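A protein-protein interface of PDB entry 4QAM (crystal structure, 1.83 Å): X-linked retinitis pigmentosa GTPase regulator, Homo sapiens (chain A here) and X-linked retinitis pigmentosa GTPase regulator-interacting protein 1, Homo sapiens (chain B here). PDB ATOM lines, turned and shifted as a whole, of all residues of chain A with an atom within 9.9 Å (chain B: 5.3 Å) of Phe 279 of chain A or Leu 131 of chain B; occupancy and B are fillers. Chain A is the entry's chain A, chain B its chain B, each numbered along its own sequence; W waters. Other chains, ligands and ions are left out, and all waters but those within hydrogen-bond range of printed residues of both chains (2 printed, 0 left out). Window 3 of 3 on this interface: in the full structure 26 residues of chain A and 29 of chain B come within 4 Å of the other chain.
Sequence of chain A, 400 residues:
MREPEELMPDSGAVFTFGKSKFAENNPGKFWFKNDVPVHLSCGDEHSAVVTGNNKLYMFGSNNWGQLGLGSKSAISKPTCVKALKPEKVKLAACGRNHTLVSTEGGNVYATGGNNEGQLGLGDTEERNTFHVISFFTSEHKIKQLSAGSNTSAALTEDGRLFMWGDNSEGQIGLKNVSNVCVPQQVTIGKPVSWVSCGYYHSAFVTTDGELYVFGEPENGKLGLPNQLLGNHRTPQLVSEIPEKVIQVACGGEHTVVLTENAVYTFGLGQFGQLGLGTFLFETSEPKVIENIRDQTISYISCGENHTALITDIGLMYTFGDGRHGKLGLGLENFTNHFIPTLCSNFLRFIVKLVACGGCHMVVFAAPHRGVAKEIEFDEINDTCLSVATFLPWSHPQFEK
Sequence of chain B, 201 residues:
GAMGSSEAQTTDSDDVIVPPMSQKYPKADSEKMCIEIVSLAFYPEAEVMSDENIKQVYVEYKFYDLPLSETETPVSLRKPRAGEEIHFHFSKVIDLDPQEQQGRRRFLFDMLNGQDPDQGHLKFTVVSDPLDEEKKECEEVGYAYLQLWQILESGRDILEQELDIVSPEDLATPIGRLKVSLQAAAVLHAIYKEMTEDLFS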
ATOM      1  N   GLY A 269       1.352   1.707 -11.116  1.00  0.00           N
ATOM      2  CA  GLY A 269       1.862   1.688  -9.731  1.00  0.00           C
ATOM      3  C   GLY A 269       3.144   2.463  -9.467  1.00  0.00           C
ATOM      4  O   GLY A 269       4.153   1.889  -9.030  1.00  0.00           O
ATOM      5  N   GLN A 270       3.025   3.804  -9.615  1.00  0.00           N
ATOM      6  CA  GLN A 270       4.226   4.680  -9.455  1.00  0.00           C
ATOM      7  C   GLN A 270       4.681   4.658  -7.990  1.00  0.00           C
ATOM      8  O   GLN A 270       5.852   5.004  -7.724  1.00  0.00           O
ATOM      9  CB  GLN A 270       3.931   6.184  -9.829  1.00  0.00           C
ATOM     10  CG  GLN A 270       2.693   6.357 -10.644  1.00  0.00           C
ATOM     11  CD  GLN A 270       1.396   6.377  -9.871  1.00  0.00           C
ATOM     12  OE1 GLN A 270       0.695   5.327  -9.694  1.00  0.00           O
ATOM     13  NE2 GLN A 270       0.915   7.624  -9.651  1.00  0.00           N
ATOM     14  N   GLY A 272       4.266   1.917  -5.966  1.00  0.00           N
ATOM     15  CA  GLY A 272       4.442   0.501  -5.412  1.00  0.00           C
ATOM     16  C   GLY A 272       3.155  -0.319  -5.287  1.00  0.00           C
ATOM     17  O   GLY A 272       3.223  -1.500  -4.900  1.00  0.00           O
ATOM     18  N   LEU A 274       1.216  -1.761  -7.328  1.00  0.00           N
ATOM     19  CA  LEU A 274       1.009  -3.013  -8.050  1.00  0.00           C
ATOM     20  C   LEU A 274       1.777  -4.137  -7.398  1.00  0.00           C
ATOM     21  O   LEU A 274       1.470  -5.349  -7.653  1.00  0.00           O
ATOM     22  CB  LEU A 274       1.518  -2.863  -9.507  1.00  0.00           C
ATOM     23  CG  LEU A 274       0.876  -1.756 -10.391  1.00  0.00           C
ATOM     24  CD1 LEU A 274       1.588  -1.898 -11.781  1.00  0.00           C
ATOM     25  CD2 LEU A 274      -0.656  -2.020 -10.571  1.00  0.00           C
ATOM     26  N   GLY A 275       2.753  -3.788  -6.530  1.00  0.00           N
ATOM     27  CA  GLY A 275       3.551  -4.834  -5.764  1.00  0.00           C
ATOM     28  C   GLY A 275       4.371  -5.722  -6.692  1.00  0.00           C
ATOM     29  O   GLY A 275       4.736  -6.892  -6.278  1.00  0.00           O
ATOM     30  N   LEU A 276       4.840  -5.150  -7.821  1.00  0.00           N
ATOM     31  CA  LEU A 276       5.612  -5.930  -8.807  1.00  0.00           C
ATOM     32  C   LEU A 276       7.077  -5.568  -8.745  1.00  0.00           C
ATOM     33  O   LEU A 276       7.817  -5.947  -9.651  1.00  0.00           O
ATOM     34  CB  LEU A 276       5.067  -5.667 -10.262  1.00  0.00           C
ATOM     35  CG  LEU A 276       3.606  -6.164 -10.423  1.00  0.00           C
ATOM     36  CD1 LEU A 276       3.051  -5.631 -11.785  1.00  0.00           C
ATOM     37  CD2 LEU A 276       3.406  -7.717 -10.306  1.00  0.00           C
ATOM     38  N   GLY A 277       7.512  -4.849  -7.679  1.00  0.00           N
ATOM     39  CA  GLY A 277       9.011  -4.671  -7.494  1.00  0.00           C
ATOM     40  C   GLY A 277       9.415  -3.249  -7.931  1.00  0.00           C
ATOM     41  O   GLY A 277       8.536  -2.416  -8.292  1.00  0.00           O
ATOM     42  N   THR A 278      10.716  -2.973  -7.839  1.00  0.00           N
ATOM     43  CA  THR A 278      11.157  -1.576  -8.050  1.00  0.00           C
ATOM     44  C   THR A 278      11.522  -1.191  -9.466  1.00  0.00           C
ATOM     45  O   THR A 278      12.195  -0.143  -9.663  1.00  0.00           O
ATOM     46  CB  THR A 278      12.397  -1.415  -7.121  1.00  0.00           C
ATOM     47  OG1 THR A 278      13.332  -2.433  -7.503  1.00  0.00           O
ATOM     48  CG2 THR A 278      11.931  -1.611  -5.612  1.00  0.00           C
ATOM     49  N   PHE A 279      11.232  -2.065 -10.459  1.00  0.00           N
ATOM     50  CA  PHE A 279      11.506  -1.792 -11.861  1.00  0.00           C
ATOM     51  C   PHE A 279      10.231  -1.674 -12.704  1.00  0.00           C
ATOM     52  O   PHE A 279      10.294  -1.136 -13.787  1.00  0.00           O
ATOM     53  CB  PHE A 279      12.388  -2.843 -12.530  1.00  0.00           C
ATOM     54  CG  PHE A 279      13.837  -2.741 -12.095  1.00  0.00           C
ATOM     55  CD1 PHE A 279      14.213  -3.080 -10.805  1.00  0.00           C
ATOM     56  CD2 PHE A 279      14.799  -2.270 -12.977  1.00  0.00           C
ATOM     57  CE1 PHE A 279      15.570  -2.963 -10.407  1.00  0.00           C
ATOM     58  CE2 PHE A 279      16.158  -2.144 -12.586  1.00  0.00           C
ATOM     59  CZ  PHE A 279      16.512  -2.427 -11.279  1.00  0.00           C
ATOM     60  N   LEU A 280       9.107  -2.220 -12.262  1.00  0.00           N
ATOM     61  CA  LEU A 280       7.985  -2.272 -13.209  1.00  0.00           C
ATOM     62  C   LEU A 280       6.877  -1.451 -12.509  1.00  0.00           C
ATOM     63  O   LEU A 280       6.339  -1.863 -11.447  1.00  0.00           O
ATOM     64  CB  LEU A 280       7.626  -3.767 -13.419  1.00  0.00           C
ATOM     65  CG  LEU A 280       6.399  -3.905 -14.371  1.00  0.00           C
ATOM     66  CD1 LEU A 280       6.871  -3.360 -15.700  1.00  0.00           C
ATOM     67  CD2 LEU A 280       5.959  -5.356 -14.555  1.00  0.00           C
ATOM     68  N   PHE A 281       6.518  -0.323 -13.079  1.00  0.00           N
ATOM     69  CA  PHE A 281       5.537   0.563 -12.418  1.00  0.00           C
ATOM     70  C   PHE A 281       4.174   0.578 -13.126  1.00  0.00           C
ATOM     71  O   PHE A 281       3.262   1.242 -12.666  1.00  0.00           O
ATOM     72  CB  PHE A 281       6.077   1.976 -12.309  1.00  0.00           C
ATOM     73  CG  PHE A 281       7.421   2.044 -11.636  1.00  0.00           C
ATOM     74  CD1 PHE A 281       7.635   1.383 -10.384  1.00  0.00           C
ATOM     75  CD2 PHE A 281       8.475   2.639 -12.264  1.00  0.00           C
ATOM     76  CE1 PHE A 281       8.953   1.374  -9.771  1.00  0.00           C
ATOM     77  CE2 PHE A 281       9.783   2.630 -11.651  1.00  0.00           C
ATOM     78  CZ  PHE A 281       9.978   2.040 -10.378  1.00  0.00           C
ATOM     79  N   GLU A 282       4.036  -0.142 -14.221  1.00  0.00           N
ATOM     80  CA  GLU A 282       2.743  -0.073 -14.953  1.00  0.00           C
ATOM     81  C   GLU A 282       2.596  -1.357 -15.674  1.00  0.00           C
ATOM     82  O   GLU A 282       3.617  -1.973 -16.066  1.00  0.00           O
ATOM     83  CB  GLU A 282       2.700   1.168 -15.892  1.00  0.00           C
ATOM     84  CG  GLU A 282       3.663   1.120 -17.147  1.00  0.00           C
ATOM     85  CD  GLU A 282       3.282   0.106 -18.277  1.00  0.00           C
ATOM     86  OE1 GLU A 282       4.216  -0.370 -18.975  1.00  0.00           O
ATOM     87  OE2 GLU A 282       2.083  -0.260 -18.516  1.00  0.00           O
ATOM     88  N   THR A 283       1.360  -1.869 -15.828  1.00  0.00           N
ATOM     89  CA  THR A 283       1.175  -2.988 -16.738  1.00  0.00           C
ATOM     90  C   THR A 283      -0.262  -2.891 -17.277  1.00  0.00           C
ATOM     91  O   THR A 283      -1.192  -2.709 -16.478  1.00  0.00           O
ATOM     92  CB  THR A 283       1.454  -4.394 -16.130  1.00  0.00           C
ATOM     93  OG1 THR A 283       1.230  -5.419 -17.130  1.00  0.00           O
ATOM     94  CG2 THR A 283       0.597  -4.712 -14.830  1.00  0.00           C
ATOM     95  N   LYS A 287      -0.787  -9.047 -14.237  1.00  0.00           N
ATOM     96  CA  LYS A 287       0.461  -9.781 -13.938  1.00  0.00           C
ATOM     97  C   LYS A 287       0.332 -10.332 -12.537  1.00  0.00           C
ATOM     98  O   LYS A 287      -0.193  -9.661 -11.678  1.00  0.00           O
ATOM     99  CB  LYS A 287       1.656  -8.807 -13.946  1.00  0.00           C
ATOM    100  CG  LYS A 287       2.107  -8.505 -15.382  1.00  0.00           C
ATOM    101  CD  LYS A 287       3.454  -7.750 -15.507  1.00  0.00           C
ATOM    102  CE  LYS A 287       4.004  -7.897 -16.977  1.00  0.00           C
ATOM    103  NZ  LYS A 287       2.925  -7.505 -17.978  1.00  0.00           N
ATOM    104  N   ASN A 291       5.761 -12.459  -5.837  1.00  0.00           N
ATOM    105  CA  ASN A 291       6.338 -12.142  -4.545  1.00  0.00           C
ATOM    106  C   ASN A 291       5.638 -12.896  -3.358  1.00  0.00           C
ATOM    107  O   ASN A 291       6.281 -13.320  -2.402  1.00  0.00           O
ATOM    108  CB  ASN A 291       6.305 -10.595  -4.416  1.00  0.00           C
ATOM    109  CG  ASN A 291       6.953  -9.885  -5.630  1.00  0.00           C
ATOM    110  OD1 ASN A 291       6.318  -9.116  -6.396  1.00  0.00           O
ATOM    111  ND2 ASN A 291       8.240 -10.170  -5.820  1.00  0.00           N
ATOM    112  N   HIS A 337       6.391   1.316  -0.624  1.00  0.00           N
ATOM    113  CA  HIS A 337       6.832  -0.101  -0.691  1.00  0.00           C
ATOM    114  C   HIS A 337       6.370  -0.725  -1.980  1.00  0.00           C
ATOM    115  O   HIS A 337       5.216  -0.535  -2.340  1.00  0.00           O
ATOM    116  CB  HIS A 337       6.141  -0.834   0.529  1.00  0.00           C
ATOM    117  CG  HIS A 337       6.842  -0.574   1.833  1.00  0.00           C
ATOM    118  ND1 HIS A 337       7.777  -1.381   2.331  1.00  0.00           N
ATOM    119  CD2 HIS A 337       6.780   0.514   2.689  1.00  0.00           C
ATOM    120  CE1 HIS A 337       8.284  -0.860   3.512  1.00  0.00           C
ATOM    121  NE2 HIS A 337       7.640   0.252   3.758  1.00  0.00           N
ATOM    122  N   PHE A 338       7.288  -1.398  -2.675  1.00  0.00           N
ATOM    123  CA  PHE A 338       7.061  -1.850  -4.076  1.00  0.00           C
ATOM    124  C   PHE A 338       6.782  -3.357  -4.254  1.00  0.00           C
ATOM    125  O   PHE A 338       6.520  -3.855  -5.384  1.00  0.00           O
ATOM    126  CB  PHE A 338       8.241  -1.419  -4.939  1.00  0.00           C
ATOM    127  CG  PHE A 338       8.196   0.093  -5.230  1.00  0.00           C
ATOM    128  CD1 PHE A 338       8.678   0.979  -4.268  1.00  0.00           C
ATOM    129  CD2 PHE A 338       7.605   0.604  -6.397  1.00  0.00           C
ATOM    130  CE1 PHE A 338       8.596   2.378  -4.481  1.00  0.00           C
ATOM    131  CE2 PHE A 338       7.490   2.035  -6.618  1.00  0.00           C
ATOM    132  CZ  PHE A 338       8.009   2.884  -5.646  1.00  0.00           C
ATOM    133  N   ILE A 339       6.937  -4.064  -3.155  1.00  0.00           N
ATOM    134  CA  ILE A 339       6.499  -5.444  -3.038  1.00  0.00           C
ATOM    135  C   ILE A 339       5.644  -5.610  -1.752  1.00  0.00           C
ATOM    136  O   ILE A 339       5.767  -4.848  -0.728  1.00  0.00           O
ATOM    137  CB  ILE A 339       7.698  -6.413  -3.029  1.00  0.00           C
ATOM    138  CG1 ILE A 339       8.539  -6.217  -1.735  1.00  0.00           C
ATOM    139  CG2 ILE A 339       8.590  -6.300  -4.350  1.00  0.00           C
ATOM    140  CD1 ILE A 339       9.773  -7.236  -1.657  1.00  0.00           C
ATOM    141  N   LYS B  55      21.710   1.511 -13.274  1.00  0.00           N
ATOM    142  CA  LYS B  55      20.396   0.865 -13.450  1.00  0.00           C
ATOM    143  C   LYS B  55      19.294   1.388 -12.471  1.00  0.00           C
ATOM    144  O   LYS B  55      18.082   1.303 -12.811  1.00  0.00           O
ATOM    145  CB  LYS B  55      20.534  -0.669 -13.356  1.00  0.00           C
ATOM    146  CG  LYS B  55      21.489  -1.191 -14.430  1.00  0.00           C
ATOM    147  CD  LYS B  55      21.280  -2.707 -14.611  1.00  0.00           C
ATOM    148  CE  LYS B  55      21.671  -3.178 -16.018  1.00  0.00           C
ATOM    149  NZ  LYS B  55      23.135  -2.885 -16.133  1.00  0.00           N
ATOM    150  N   GLN B  56      19.677   1.836 -11.293  1.00  0.00           N
ATOM    151  CA  GLN B  56      18.702   2.171 -10.259  1.00  0.00           C
ATOM    152  C   GLN B  56      19.404   3.146  -9.360  1.00  0.00           C
ATOM    153  O   GLN B  56      20.666   3.157  -9.302  1.00  0.00           O
ATOM    154  CB  GLN B  56      18.209   0.882  -9.481  1.00  0.00           C
ATOM    155  CG  GLN B  56      19.395   0.124  -8.879  1.00  0.00           C
ATOM    156  CD  GLN B  56      18.975  -1.120  -8.112  1.00  0.00           C
ATOM    157  OE1 GLN B  56      17.788  -1.473  -8.053  1.00  0.00           O
ATOM    158  NE2 GLN B  56      19.948  -1.733  -7.439  1.00  0.00           N
ATOM    159  N   ARG B  78      14.366   1.800 -10.220  1.00  0.00           N
ATOM    160  CA  ARG B  78      14.853   1.876 -11.586  1.00  0.00           C
ATOM    161  C   ARG B  78      15.087   3.326 -12.048  1.00  0.00           C
ATOM    162  O   ARG B  78      14.218   4.192 -11.873  1.00  0.00           O
ATOM    163  CB  ARG B  78      13.816   1.228 -12.546  1.00  0.00           C
ATOM    164  CG  ARG B  78      14.310   1.308 -13.972  1.00  0.00           C
ATOM    165  CD  ARG B  78      13.316   0.600 -14.885  1.00  0.00           C
ATOM    166  NE  ARG B  78      11.916   0.992 -14.713  1.00  0.00           N
ATOM    167  CZ  ARG B  78      11.346   2.101 -15.239  1.00  0.00           C
ATOM    168  NH1 ARG B  78      12.104   3.071 -15.765  1.00  0.00           N
ATOM    169  NH2 ARG B  78      10.022   2.311 -15.156  1.00  0.00           N
ATOM    170  N   ASP B 129      22.957   2.589  -7.369  1.00  0.00           N
ATOM    171  CA  ASP B 129      23.074   1.383  -6.510  1.00  0.00           C
ATOM    172  C   ASP B 129      23.226   0.212  -7.459  1.00  0.00           C
ATOM    173  O   ASP B 129      22.331  -0.037  -8.193  1.00  0.00           O
ATOM    174  CB  ASP B 129      21.774   1.283  -5.734  1.00  0.00           C
ATOM    175  CG  ASP B 129      21.877   0.349  -4.543  1.00  0.00           C
ATOM    176  OD1 ASP B 129      23.005  -0.054  -4.181  1.00  0.00           O
ATOM    177  OD2 ASP B 129      20.808   0.020  -3.983  1.00  0.00           O
ATOM    178  N   PRO B 130      24.369  -0.507  -7.441  1.00  0.00           N
ATOM    179  CA  PRO B 130      24.542  -1.657  -8.327  1.00  0.00           C
ATOM    180  C   PRO B 130      23.474  -2.716  -7.982  1.00  0.00           C
ATOM    181  O   PRO B 130      22.950  -2.747  -6.882  1.00  0.00           O
ATOM    182  CB  PRO B 130      25.915  -2.250  -7.886  1.00  0.00           C
ATOM    183  CG  PRO B 130      26.585  -1.134  -7.141  1.00  0.00           C
ATOM    184  CD  PRO B 130      25.505  -0.350  -6.502  1.00  0.00           C
ATOM    185  N   LEU B 131      23.192  -3.657  -8.898  1.00  0.00           N
ATOM    186  CA  LEU B 131      22.101  -4.606  -8.599  1.00  0.00           C
ATOM    187  C   LEU B 131      22.524  -5.487  -7.412  1.00  0.00           C
ATOM    188  O   LEU B 131      21.723  -5.880  -6.551  1.00  0.00           O
ATOM    189  CB  LEU B 131      21.890  -5.522  -9.857  1.00  0.00           C
ATOM    190  CG  LEU B 131      21.301  -4.706 -11.059  1.00  0.00           C
ATOM    191  CD1 LEU B 131      21.219  -5.513 -12.367  1.00  0.00           C
ATOM    192  CD2 LEU B 131      19.907  -4.156 -10.616  1.00  0.00           C
ATOM    193  N   ASP B 132      23.826  -5.713  -7.324  1.00  0.00           N
ATOM    194  CA  ASP B 132      24.348  -6.484  -6.165  1.00  0.00           C
ATOM    195  C   ASP B 132      24.530  -5.624  -4.900  1.00  0.00           C
ATOM    196  O   ASP B 132      24.932  -6.158  -3.870  1.00  0.00           O
ATOM    197  CB  ASP B 132      25.617  -7.304  -6.513  1.00  0.00           C
ATOM    198  CG  ASP B 132      26.868  -6.411  -6.793  1.00  0.00           C
ATOM    199  OD1 ASP B 132      26.845  -5.151  -6.598  1.00  0.00           O
ATOM    200  OD2 ASP B 132      27.899  -6.935  -7.277  1.00  0.00           O
ATOM    201  N   GLU B 133      24.225  -4.336  -4.966  1.00  0.00           N
ATOM    202  CA  GLU B 133      24.188  -3.475  -3.760  1.00  0.00           C
ATOM    203  C   GLU B 133      25.568  -3.322  -3.078  1.00  0.00           C
ATOM    204  O   GLU B 133      25.667  -2.898  -1.927  1.00  0.00           O
ATOM    205  CB  GLU B 133      23.175  -3.950  -2.754  1.00  0.00           C
ATOM    206  CG  GLU B 133      21.751  -3.884  -3.290  1.00  0.00           C
ATOM    207  CD  GLU B 133      20.762  -4.287  -2.183  1.00  0.00           C
ATOM    208  OE1 GLU B 133      20.760  -5.460  -1.759  1.00  0.00           O
ATOM    209  OE2 GLU B 133      20.064  -3.412  -1.649  1.00  0.00           O
HETATM  210  O   HOH W   1       7.407   0.680 -15.767  1.00  0.00           O
HETATM  211  O   HOH W   2      15.833  -2.024  -6.018  1.00  0.00           O
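The backbone carbonyl oxygen (O) of Phe 279 of chain A sits at hydrogen-bond distance from the guanidinium group (NE) of Arg 78 of chain B (2.8 Å). The backbone NH (N) of Arg 78 of chain B sits at hydrogen-bond distance from the backbone carbonyl oxygen (O) of Thr 278 of chain A (3.0 Å).
Among the printed residues, merely in contact across the chains: Phe 279 of chain A with Lys 55 of chain B (3.95 Å), Phe 279 of chain A with Gln 56 of chain B (3.6 Å), Phe 279 of chain A with Leu 131 of chain B (3.9 Å) and Phe 281 of chain A with Arg 78 of chain B (3.3 Å).
Of the 8 printed residues of chain B, 4 touch a printed residue of chain A. Of the 18 printed residues of chain A, 3 touch a printed residue of chain B. Hydrophobic or aromatic side chains of chain A within 4 Å of the printed part of chain B: Phe 279 and Phe 281. Among the printed residues, 6 pairs touch across the chains. Among the printed residues, no Asp or Glu carboxylate lies within 4 Å of a Lys or Arg side-chain nitrogen of the other chain.
N of Gly 269 of chain A lies within hydrogen-bond range of O of Phe 281 of chain A (2.5 Å). NE2 of Gln 56 of chain B lies within hydrogen-bond range of O of Pro 130 of chain B (3.2 Å). NE2 of Gln 56 of chain B sits close to O of Asp 129 of chain B (3.0 Å).
Water W2 lies within hydrogen-bond range of OE1 of Gln 56 of chain B (2.9 Å) and OG1 of Thr 278 of chain A (2.9 Å). Water W1 bridges the backbone NH (N) of Phe 281 of chain A (3.0 Å) and the guanidinium group (NH2) of Arg 78 of chain B (3.1 Å).
Printed residues of chain B within 4 Å of Phe 279 of chain A: Lys 55 (3.95 Å), Gln 56 (3.6 Å), Arg 78 (2.8 Å) and Leu 131 (3.9 Å). Leu 131 of chain B touches just one residue of chain A: Phe 279. No residue of chain A comes within 4 Å of Pro 130 of chain B. Of the printed residues of chain A, Gln 56 of chain B touches Phe 279 (3.6 Å). Printed residues of chain B within 4 Å of Phe 281 of chain A: Arg 78. Printed residues of chain A within 4 Å of Lys 55 of chain B: Phe 279. The nearest printed residue of chain B that does not touch Phe 279 of chain A is Asp 129 of chain B (7.0 Å). The nearest residue of chain A that does not touch Leu 131 of chain B is Thr 278 of chain A (7.5 Å).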
